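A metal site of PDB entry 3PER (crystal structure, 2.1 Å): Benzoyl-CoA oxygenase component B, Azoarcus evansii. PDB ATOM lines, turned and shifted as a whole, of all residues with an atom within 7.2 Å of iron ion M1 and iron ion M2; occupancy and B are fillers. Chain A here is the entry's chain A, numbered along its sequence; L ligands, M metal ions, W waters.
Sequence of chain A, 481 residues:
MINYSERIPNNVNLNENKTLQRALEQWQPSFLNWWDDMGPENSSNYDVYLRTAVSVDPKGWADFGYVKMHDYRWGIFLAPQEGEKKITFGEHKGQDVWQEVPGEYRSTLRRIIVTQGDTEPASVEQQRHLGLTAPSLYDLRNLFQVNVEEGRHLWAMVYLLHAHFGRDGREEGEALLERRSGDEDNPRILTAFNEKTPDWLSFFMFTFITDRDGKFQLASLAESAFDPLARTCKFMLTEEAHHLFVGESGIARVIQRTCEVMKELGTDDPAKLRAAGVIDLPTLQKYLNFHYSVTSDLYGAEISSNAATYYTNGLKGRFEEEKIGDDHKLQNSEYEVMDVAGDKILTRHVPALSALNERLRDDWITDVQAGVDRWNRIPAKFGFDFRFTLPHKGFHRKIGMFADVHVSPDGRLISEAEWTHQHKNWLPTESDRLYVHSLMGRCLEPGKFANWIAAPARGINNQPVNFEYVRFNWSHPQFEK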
ATOM      1  N   GLN A 116       9.642 -25.289 -14.260  1.00  0.00           N
ATOM      2  CA  GLN A 116       8.222 -25.015 -14.075  1.00  0.00           C
ATOM      3  C   GLN A 116       7.549 -24.677 -15.436  1.00  0.00           C
ATOM      4  O   GLN A 116       6.453 -25.162 -15.743  1.00  0.00           O
ATOM      5  CB  GLN A 116       8.035 -23.865 -13.068  1.00  0.00           C
ATOM      6  CG  GLN A 116       6.595 -23.420 -12.930  1.00  0.00           C
ATOM      7  CD  GLN A 116       5.713 -24.526 -12.380  1.00  0.00           C
ATOM      8  OE1 GLN A 116       6.156 -25.333 -11.561  1.00  0.00           O
ATOM      9  NE2 GLN A 116       4.471 -24.576 -12.845  1.00  0.00           N
ATOM     10  N   THR A 119       6.506 -27.647 -17.965  1.00  0.00           N
ATOM     11  CA  THR A 119       5.359 -28.526 -17.735  1.00  0.00           C
ATOM     12  C   THR A 119       4.095 -27.994 -18.421  1.00  0.00           C
ATOM     13  O   THR A 119       3.165 -28.743 -18.658  1.00  0.00           O
ATOM     14  CB  THR A 119       5.038 -28.657 -16.216  1.00  0.00           C
ATOM     15  OG1 THR A 119       4.602 -27.389 -15.713  1.00  0.00           O
ATOM     16  CG2 THR A 119       6.262 -29.141 -15.444  1.00  0.00           C
ATOM     17  N   GLU A 120       4.062 -26.693 -18.688  1.00  0.00           N
ATOM     18  CA  GLU A 120       2.840 -26.034 -19.142  1.00  0.00           C
ATOM     19  C   GLU A 120       2.487 -26.484 -20.586  1.00  0.00           C
ATOM     20  O   GLU A 120       1.447 -27.085 -20.798  1.00  0.00           O
ATOM     21  CB  GLU A 120       2.980 -24.517 -19.035  1.00  0.00           C
ATOM     22  CG  GLU A 120       3.585 -24.023 -17.700  1.00  0.00           C
ATOM     23  CD  GLU A 120       2.689 -24.265 -16.469  1.00  0.00           C
ATOM     24  OE1 GLU A 120       1.534 -24.680 -16.641  1.00  0.00           O
ATOM     25  OE2 GLU A 120       3.140 -24.014 -15.327  1.00  0.00           O
ATOM     26  N   SER A 123       1.674 -30.292 -20.866  1.00  0.00           N
ATOM     27  CA  SER A 123       0.328 -30.780 -20.609  1.00  0.00           C
ATOM     28  C   SER A 123      -0.579 -30.584 -21.821  1.00  0.00           C
ATOM     29  O   SER A 123      -1.466 -31.390 -22.076  1.00  0.00           O
ATOM     30  CB  SER A 123      -0.296 -30.081 -19.401  1.00  0.00           C
ATOM     31  OG  SER A 123      -0.669 -28.742 -19.709  1.00  0.00           O
ATOM     32  N   VAL A 146      -8.713 -25.308 -19.819  1.00  0.00           N
ATOM     33  CA  VAL A 146      -7.475 -25.749 -19.191  1.00  0.00           C
ATOM     34  C   VAL A 146      -6.333 -25.548 -20.163  1.00  0.00           C
ATOM     35  O   VAL A 146      -5.277 -25.039 -19.776  1.00  0.00           O
ATOM     36  CB  VAL A 146      -7.517 -27.236 -18.760  1.00  0.00           C
ATOM     37  CG1 VAL A 146      -6.114 -27.707 -18.316  1.00  0.00           C
ATOM     38  CG2 VAL A 146      -8.505 -27.432 -17.600  1.00  0.00           C
ATOM     39  N   GLU A 149      -5.262 -21.869 -20.576  1.00  0.00           N
ATOM     40  CA  GLU A 149      -4.628 -21.413 -19.335  1.00  0.00           C
ATOM     41  C   GLU A 149      -3.196 -21.959 -19.182  1.00  0.00           C
ATOM     42  O   GLU A 149      -2.299 -21.233 -18.752  1.00  0.00           O
ATOM     43  CB  GLU A 149      -5.483 -21.778 -18.127  1.00  0.00           C
ATOM     44  CG  GLU A 149      -6.749 -20.933 -18.074  1.00  0.00           C
ATOM     45  CD  GLU A 149      -7.774 -21.468 -17.103  1.00  0.00           C
ATOM     46  OE1 GLU A 149      -7.568 -22.541 -16.523  1.00  0.00           O
ATOM     47  OE2 GLU A 149      -8.801 -20.813 -16.944  1.00  0.00           O
ATOM     48  N   GLU A 150      -3.001 -23.233 -19.523  1.00  0.00           N
ATOM     49  CA  GLU A 150      -1.656 -23.811 -19.478  1.00  0.00           C
ATOM     50  C   GLU A 150      -0.783 -23.054 -20.479  1.00  0.00           C
ATOM     51  O   GLU A 150       0.393 -22.808 -20.228  1.00  0.00           O
ATOM     52  CB  GLU A 150      -1.670 -25.307 -19.798  1.00  0.00           C
ATOM     53  CG  GLU A 150      -2.519 -26.132 -18.825  1.00  0.00           C
ATOM     54  CD  GLU A 150      -2.041 -26.061 -17.353  1.00  0.00           C
ATOM     55  OE1 GLU A 150      -1.302 -25.123 -16.983  1.00  0.00           O
ATOM     56  OE2 GLU A 150      -2.405 -26.957 -16.570  1.00  0.00           O
ATOM     57  N   GLY A 151      -1.387 -22.680 -21.609  1.00  0.00           N
ATOM     58  CA  GLY A 151      -0.700 -21.845 -22.576  1.00  0.00           C
ATOM     59  C   GLY A 151      -0.288 -20.522 -21.957  1.00  0.00           C
ATOM     60  O   GLY A 151       0.799 -20.039 -22.214  1.00  0.00           O
ATOM     61  N   ARG A 152      -1.165 -19.932 -21.135  1.00  0.00           N
ATOM     62  CA  ARG A 152      -0.821 -18.691 -20.450  1.00  0.00           C
ATOM     63  C   ARG A 152       0.306 -18.867 -19.462  1.00  0.00           C
ATOM     64  O   ARG A 152       1.088 -17.951 -19.255  1.00  0.00           O
ATOM     65  CB  ARG A 152      -2.011 -18.054 -19.719  1.00  0.00           C
ATOM     66  CG  ARG A 152      -1.879 -16.507 -19.685  1.00  0.00           C
ATOM     67  CD  ARG A 152      -2.713 -15.872 -18.588  1.00  0.00           C
ATOM     68  NE  ARG A 152      -2.297 -16.359 -17.270  1.00  0.00           N
ATOM     69  CZ  ARG A 152      -1.231 -15.933 -16.592  1.00  0.00           C
ATOM     70  NH1 ARG A 152      -0.946 -16.454 -15.408  1.00  0.00           N
ATOM     71  NH2 ARG A 152      -0.458 -14.974 -17.097  1.00  0.00           N
ATOM     72  N   HIS A 153       0.393 -20.044 -18.844  1.00  0.00           N
ATOM     73  CA  HIS A 153       1.423 -20.262 -17.844  1.00  0.00           C
ATOM     74  C   HIS A 153       2.769 -20.307 -18.519  1.00  0.00           C
ATOM     75  O   HIS A 153       3.778 -19.913 -17.931  1.00  0.00           O
ATOM     76  CB  HIS A 153       1.133 -21.534 -17.021  1.00  0.00           C
ATOM     77  CG  HIS A 153      -0.050 -21.380 -16.132  1.00  0.00           C
ATOM     78  ND1 HIS A 153      -0.578 -22.421 -15.392  1.00  0.00           N
ATOM     79  CD2 HIS A 153      -0.832 -20.294 -15.872  1.00  0.00           C
ATOM     80  CE1 HIS A 153      -1.631 -21.980 -14.721  1.00  0.00           C
ATOM     81  NE2 HIS A 153      -1.817 -20.713 -15.008  1.00  0.00           N
ATOM     82  N   LEU A 154       2.806 -20.802 -19.762  1.00  0.00           N
ATOM     83  CA  LEU A 154       4.032 -20.760 -20.529  1.00  0.00           C
ATOM     84  C   LEU A 154       4.403 -19.289 -20.737  1.00  0.00           C
ATOM     85  O   LEU A 154       5.544 -18.898 -20.552  1.00  0.00           O
ATOM     86  CB  LEU A 154       3.892 -21.456 -21.886  1.00  0.00           C
ATOM     87  CG  LEU A 154       5.161 -21.330 -22.729  1.00  0.00           C
ATOM     88  CD1 LEU A 154       6.375 -21.837 -21.934  1.00  0.00           C
ATOM     89  CD2 LEU A 154       5.032 -22.035 -24.076  1.00  0.00           C
ATOM     90  N   PHE A 206      -5.346 -36.596 -14.018  1.00  0.00           N
ATOM     91  CA  PHE A 206      -4.167 -35.782 -14.200  1.00  0.00           C
ATOM     92  C   PHE A 206      -4.408 -34.375 -13.656  1.00  0.00           C
ATOM     93  O   PHE A 206      -3.558 -33.831 -12.940  1.00  0.00           O
ATOM     94  CB  PHE A 206      -3.781 -35.737 -15.682  1.00  0.00           C
ATOM     95  CG  PHE A 206      -2.486 -35.008 -15.955  1.00  0.00           C
ATOM     96  CD1 PHE A 206      -1.291 -35.712 -16.103  1.00  0.00           C
ATOM     97  CD2 PHE A 206      -2.457 -33.626 -16.046  1.00  0.00           C
ATOM     98  CE1 PHE A 206      -0.093 -35.049 -16.369  1.00  0.00           C
ATOM     99  CE2 PHE A 206      -1.273 -32.938 -16.311  1.00  0.00           C
ATOM    100  CZ  PHE A 206      -0.088 -33.656 -16.473  1.00  0.00           C
ATOM    101  N   THR A 207      -5.584 -33.807 -13.949  1.00  0.00           N
ATOM    102  CA  THR A 207      -5.889 -32.452 -13.497  1.00  0.00           C
ATOM    103  C   THR A 207      -6.234 -32.456 -11.999  1.00  0.00           C
ATOM    104  O   THR A 207      -6.081 -31.461 -11.285  1.00  0.00           O
ATOM    105  CB  THR A 207      -7.010 -31.757 -14.350  1.00  0.00           C
ATOM    106  OG1 THR A 207      -8.148 -32.624 -14.480  1.00  0.00           O
ATOM    107  CG2 THR A 207      -6.503 -31.430 -15.758  1.00  0.00           C
ATOM    108  N   THR A 210      -1.932 -34.418 -10.773  1.00  0.00           N
ATOM    109  CA  THR A 210      -0.690 -33.863 -11.294  1.00  0.00           C
ATOM    110  C   THR A 210      -0.716 -32.333 -11.362  1.00  0.00           C
ATOM    111  O   THR A 210       0.278 -31.713 -10.997  1.00  0.00           O
ATOM    112  CB  THR A 210      -0.383 -34.466 -12.672  1.00  0.00           C
ATOM    113  OG1 THR A 210      -0.509 -35.882 -12.573  1.00  0.00           O
ATOM    114  CG2 THR A 210       1.030 -34.124 -13.128  1.00  0.00           C
ATOM    115  N   ASP A 211      -1.803 -31.709 -11.815  1.00  0.00           N
ATOM    116  CA  ASP A 211      -1.895 -30.246 -11.709  1.00  0.00           C
ATOM    117  C   ASP A 211      -1.747 -29.828 -10.250  1.00  0.00           C
ATOM    118  O   ASP A 211      -1.396 -28.682  -9.954  1.00  0.00           O
ATOM    119  CB  ASP A 211      -3.214 -29.683 -12.274  1.00  0.00           C
ATOM    120  CG  ASP A 211      -3.237 -29.648 -13.820  1.00  0.00           C
ATOM    121  OD1 ASP A 211      -2.835 -30.664 -14.418  1.00  0.00           O
ATOM    122  OD2 ASP A 211      -3.651 -28.632 -14.423  1.00  0.00           O
ATOM    123  N   ARG A 212      -2.026 -30.742  -9.321  1.00  0.00           N
ATOM    124  CA  ARG A 212      -1.929 -30.386  -7.911  1.00  0.00           C
ATOM    125  C   ARG A 212      -0.464 -30.310  -7.469  1.00  0.00           C
ATOM    126  O   ARG A 212      -0.126 -29.563  -6.539  1.00  0.00           O
ATOM    127  CB  ARG A 212      -2.684 -31.375  -7.020  1.00  0.00           C
ATOM    128  CG  ARG A 212      -2.998 -30.809  -5.629  1.00  0.00           C
ATOM    129  CD  ARG A 212      -3.847 -31.786  -4.844  1.00  0.00           C
ATOM    130  NE  ARG A 212      -5.057 -32.132  -5.554  1.00  0.00           N
ATOM    131  CZ  ARG A 212      -6.228 -31.512  -5.419  1.00  0.00           C
ATOM    132  NH1 ARG A 212      -6.376 -30.508  -4.563  1.00  0.00           N
ATOM    133  NH2 ARG A 212      -7.271 -31.908  -6.150  1.00  0.00           N
ATOM    134  N   GLY A 214       1.529 -29.009  -9.522  1.00  0.00           N
ATOM    135  CA  GLY A 214       1.723 -27.637  -9.984  1.00  0.00           C
ATOM    136  C   GLY A 214       1.355 -26.662  -8.867  1.00  0.00           C
ATOM    137  O   GLY A 214       2.098 -25.737  -8.564  1.00  0.00           O
ATOM    138  N   LYS A 215       0.208 -26.883  -8.263  1.00  0.00           N
ATOM    139  CA  LYS A 215      -0.234 -26.058  -7.152  1.00  0.00           C
ATOM    140  C   LYS A 215       0.844 -25.953  -6.066  1.00  0.00           C
ATOM    141  O   LYS A 215       1.210 -24.851  -5.640  1.00  0.00           O
ATOM    142  CB  LYS A 215      -1.515 -26.621  -6.553  1.00  0.00           C
ATOM    143  CG  LYS A 215      -2.057 -25.816  -5.367  1.00  0.00           C
ATOM    144  CD  LYS A 215      -3.018 -26.654  -4.553  1.00  0.00           C
ATOM    145  CE  LYS A 215      -3.338 -26.009  -3.214  1.00  0.00           C
ATOM    146  NZ  LYS A 215      -4.633 -26.521  -2.691  1.00  0.00           N
ATOM    147  N   LEU A 218       4.056 -24.189  -7.250  1.00  0.00           N
ATOM    148  CA  LEU A 218       3.778 -22.757  -7.423  1.00  0.00           C
ATOM    149  C   LEU A 218       3.604 -22.066  -6.063  1.00  0.00           C
ATOM    150  O   LEU A 218       3.980 -20.919  -5.904  1.00  0.00           O
ATOM    151  CB  LEU A 218       2.514 -22.541  -8.276  1.00  0.00           C
ATOM    152  CG  LEU A 218       2.603 -22.918  -9.768  1.00  0.00           C
ATOM    153  CD1 LEU A 218       1.235 -22.824 -10.472  1.00  0.00           C
ATOM    154  CD2 LEU A 218       3.641 -22.036 -10.448  1.00  0.00           C
ATOM    155  N   MET A 236      -1.046 -17.349 -10.699  1.00  0.00           N
ATOM    156  CA  MET A 236      -1.272 -18.651 -11.345  1.00  0.00           C
ATOM    157  C   MET A 236      -1.990 -19.628 -10.428  1.00  0.00           C
ATOM    158  O   MET A 236      -2.634 -20.557 -10.903  1.00  0.00           O
ATOM    159  CB  MET A 236       0.056 -19.280 -11.791  1.00  0.00           C
ATOM    160  CG  MET A 236       0.693 -18.567 -12.952  1.00  0.00           C
ATOM    161  SD  MET A 236       2.418 -19.056 -13.158  1.00  0.00           S
ATOM    162  CE  MET A 236       2.182 -20.762 -13.670  1.00  0.00           C
ATOM    163  N   GLU A 239      -5.625 -19.699 -11.055  1.00  0.00           N
ATOM    164  CA  GLU A 239      -5.971 -20.445 -12.266  1.00  0.00           C
ATOM    165  C   GLU A 239      -5.860 -21.953 -12.028  1.00  0.00           C
ATOM    166  O   GLU A 239      -6.726 -22.727 -12.426  1.00  0.00           O
ATOM    167  CB  GLU A 239      -5.065 -20.051 -13.427  1.00  0.00           C
ATOM    168  CG  GLU A 239      -5.193 -18.583 -13.817  1.00  0.00           C
ATOM    169  CD  GLU A 239      -4.059 -18.133 -14.726  1.00  0.00           C
ATOM    170  OE1 GLU A 239      -2.878 -18.355 -14.366  1.00  0.00           O
ATOM    171  OE2 GLU A 239      -4.353 -17.586 -15.810  1.00  0.00           O
ATOM    172  N   GLU A 240      -4.792 -22.363 -11.372  1.00  0.00           N
ATOM    173  CA  GLU A 240      -4.581 -23.773 -11.047  1.00  0.00           C
ATOM    174  C   GLU A 240      -5.781 -24.340 -10.293  1.00  0.00           C
ATOM    175  O   GLU A 240      -6.086 -25.512 -10.422  1.00  0.00           O
ATOM    176  CB  GLU A 240      -3.320 -23.932 -10.218  1.00  0.00           C
ATOM    177  CG  GLU A 240      -2.862 -25.365 -10.074  1.00  0.00           C
ATOM    178  CD  GLU A 240      -2.237 -25.914 -11.345  1.00  0.00           C
ATOM    179  OE1 GLU A 240      -0.980 -25.917 -11.454  1.00  0.00           O
ATOM    180  OE2 GLU A 240      -2.998 -26.337 -12.249  1.00  0.00           O
ATOM    181  N   ALA A 241      -6.447 -23.518  -9.495  1.00  0.00           N
ATOM    182  CA  ALA A 241      -7.647 -23.954  -8.764  1.00  0.00           C
ATOM    183  C   ALA A 241      -8.742 -24.466  -9.702  1.00  0.00           C
ATOM    184  O   ALA A 241      -9.450 -25.432  -9.396  1.00  0.00           O
ATOM    185  CB  ALA A 241      -8.197 -22.818  -7.899  1.00  0.00           C
ATOM    186  N   HIS A 243      -8.294 -25.841 -12.630  1.00  0.00           N
ATOM    187  CA  HIS A 243      -7.848 -27.127 -13.178  1.00  0.00           C
ATOM    188  C   HIS A 243      -8.169 -28.265 -12.204  1.00  0.00           C
ATOM    189  O   HIS A 243      -8.646 -29.335 -12.597  1.00  0.00           O
ATOM    190  CB  HIS A 243      -6.341 -27.103 -13.448  1.00  0.00           C
ATOM    191  CG  HIS A 243      -5.920 -26.038 -14.393  1.00  0.00           C
ATOM    192  ND1 HIS A 243      -4.611 -25.857 -14.780  1.00  0.00           N
ATOM    193  CD2 HIS A 243      -6.634 -25.075 -15.033  1.00  0.00           C
ATOM    194  CE1 HIS A 243      -4.528 -24.830 -15.612  1.00  0.00           C
ATOM    195  NE2 HIS A 243      -5.743 -24.329 -15.777  1.00  0.00           N
ATOM    196  N   LEU A 244      -7.910 -28.006 -10.927  1.00  0.00           N
ATOM    197  CA  LEU A 244      -8.130 -28.988  -9.883  1.00  0.00           C
ATOM    198  C   LEU A 244      -9.622 -29.270  -9.792  1.00  0.00           C
ATOM    199  O   LEU A 244     -10.033 -30.397  -9.541  1.00  0.00           O
ATOM    200  CB  LEU A 244      -7.610 -28.461  -8.561  1.00  0.00           C
ATOM    201  CG  LEU A 244      -6.101 -28.229  -8.511  1.00  0.00           C
ATOM    202  CD1 LEU A 244      -5.724 -27.673  -7.151  1.00  0.00           C
ATOM    203  CD2 LEU A 244      -5.315 -29.492  -8.784  1.00  0.00           C
HETATM  204  O1  LIG L   1      -1.423 -24.851 -14.116  1.00  0.00           O
HETATM  205  P1  LG2 L   2       0.301 -27.996 -14.596  1.00  0.00           P
HETATM  206  O1  LG2 L   2      -0.192 -29.005 -15.622  1.00  0.00           O
HETATM  207  O2  LG2 L   2      -0.828 -27.489 -13.746  1.00  0.00           O
HETATM  208  O3  LG2 L   2       1.335 -28.660 -13.732  1.00  0.00           O
HETATM  209  O4  LG2 L   2       0.922 -26.841 -15.364  1.00  0.00           O
HETATM  210 FE    FE M   1      -2.661 -26.694 -14.354  1.00  0.00          FE
HETATM  211 FE    FE M   2      -0.001 -24.645 -15.292  1.00  0.00          FE
HETATM  212  O   HOH W   1       1.388 -24.477 -13.551  1.00  0.00           O
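OE2 of Glu 120 sits at hydrogen-bond distance from NE2 of Gln 116, at 2.9 Å.
The backbone carbonyl oxygen of Glu 120 lies within hydrogen-bond range of the side-chain hydroxyl of Ser 123.
OE1 of Glu 149 lies within hydrogen-bond range of NE2 of His 243 (2.7 Å).
O of Phe 206 lies within hydrogen-bond range of N of Asp 211, at 3.0 Å.
The side-chain carboxylate (OE1) of Glu 239 is in hydrogen-bond range of a ring nitrogen (NE2) of His 153 (2.7 Å).
Within 4 Å of iron ion M1: Glu 150, Asp 211, Glu 240 and His 243.
The nearest printed residue that does not touch iron ion M1 is His 153 (4.8 Å).
Of the 25 residues printed, 3 come within 4 Å of iron ion M2.
Iron ion M1 is bound by O2 of LG2 L2 (2.1 Å), OE2 of Glu 240 (2.2 Å), ND1 of His 243 (2.2 Å), OD2 of Asp 211 (2.2 Å), O1 of LIG L1 (2.2 Å) and OE2 of Glu 150 (2.2 Å).
Iron ion M2 is bound by an oxygen (O1) of LIG L1, the side-chain carboxylate of Glu 120, the side-chain carboxylate of Glu 150, water W1, a ring nitrogen (ND1) of His 153 and an oxygen (O4) of LG2 L2.
Water W1 lies within hydrogen-bond range of the side-chain carboxylate (OE2) of Glu 120, the side-chain amide nitrogen (NE2) of Gln 116 and the side-chain carboxylate (OE1) of Glu 240.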
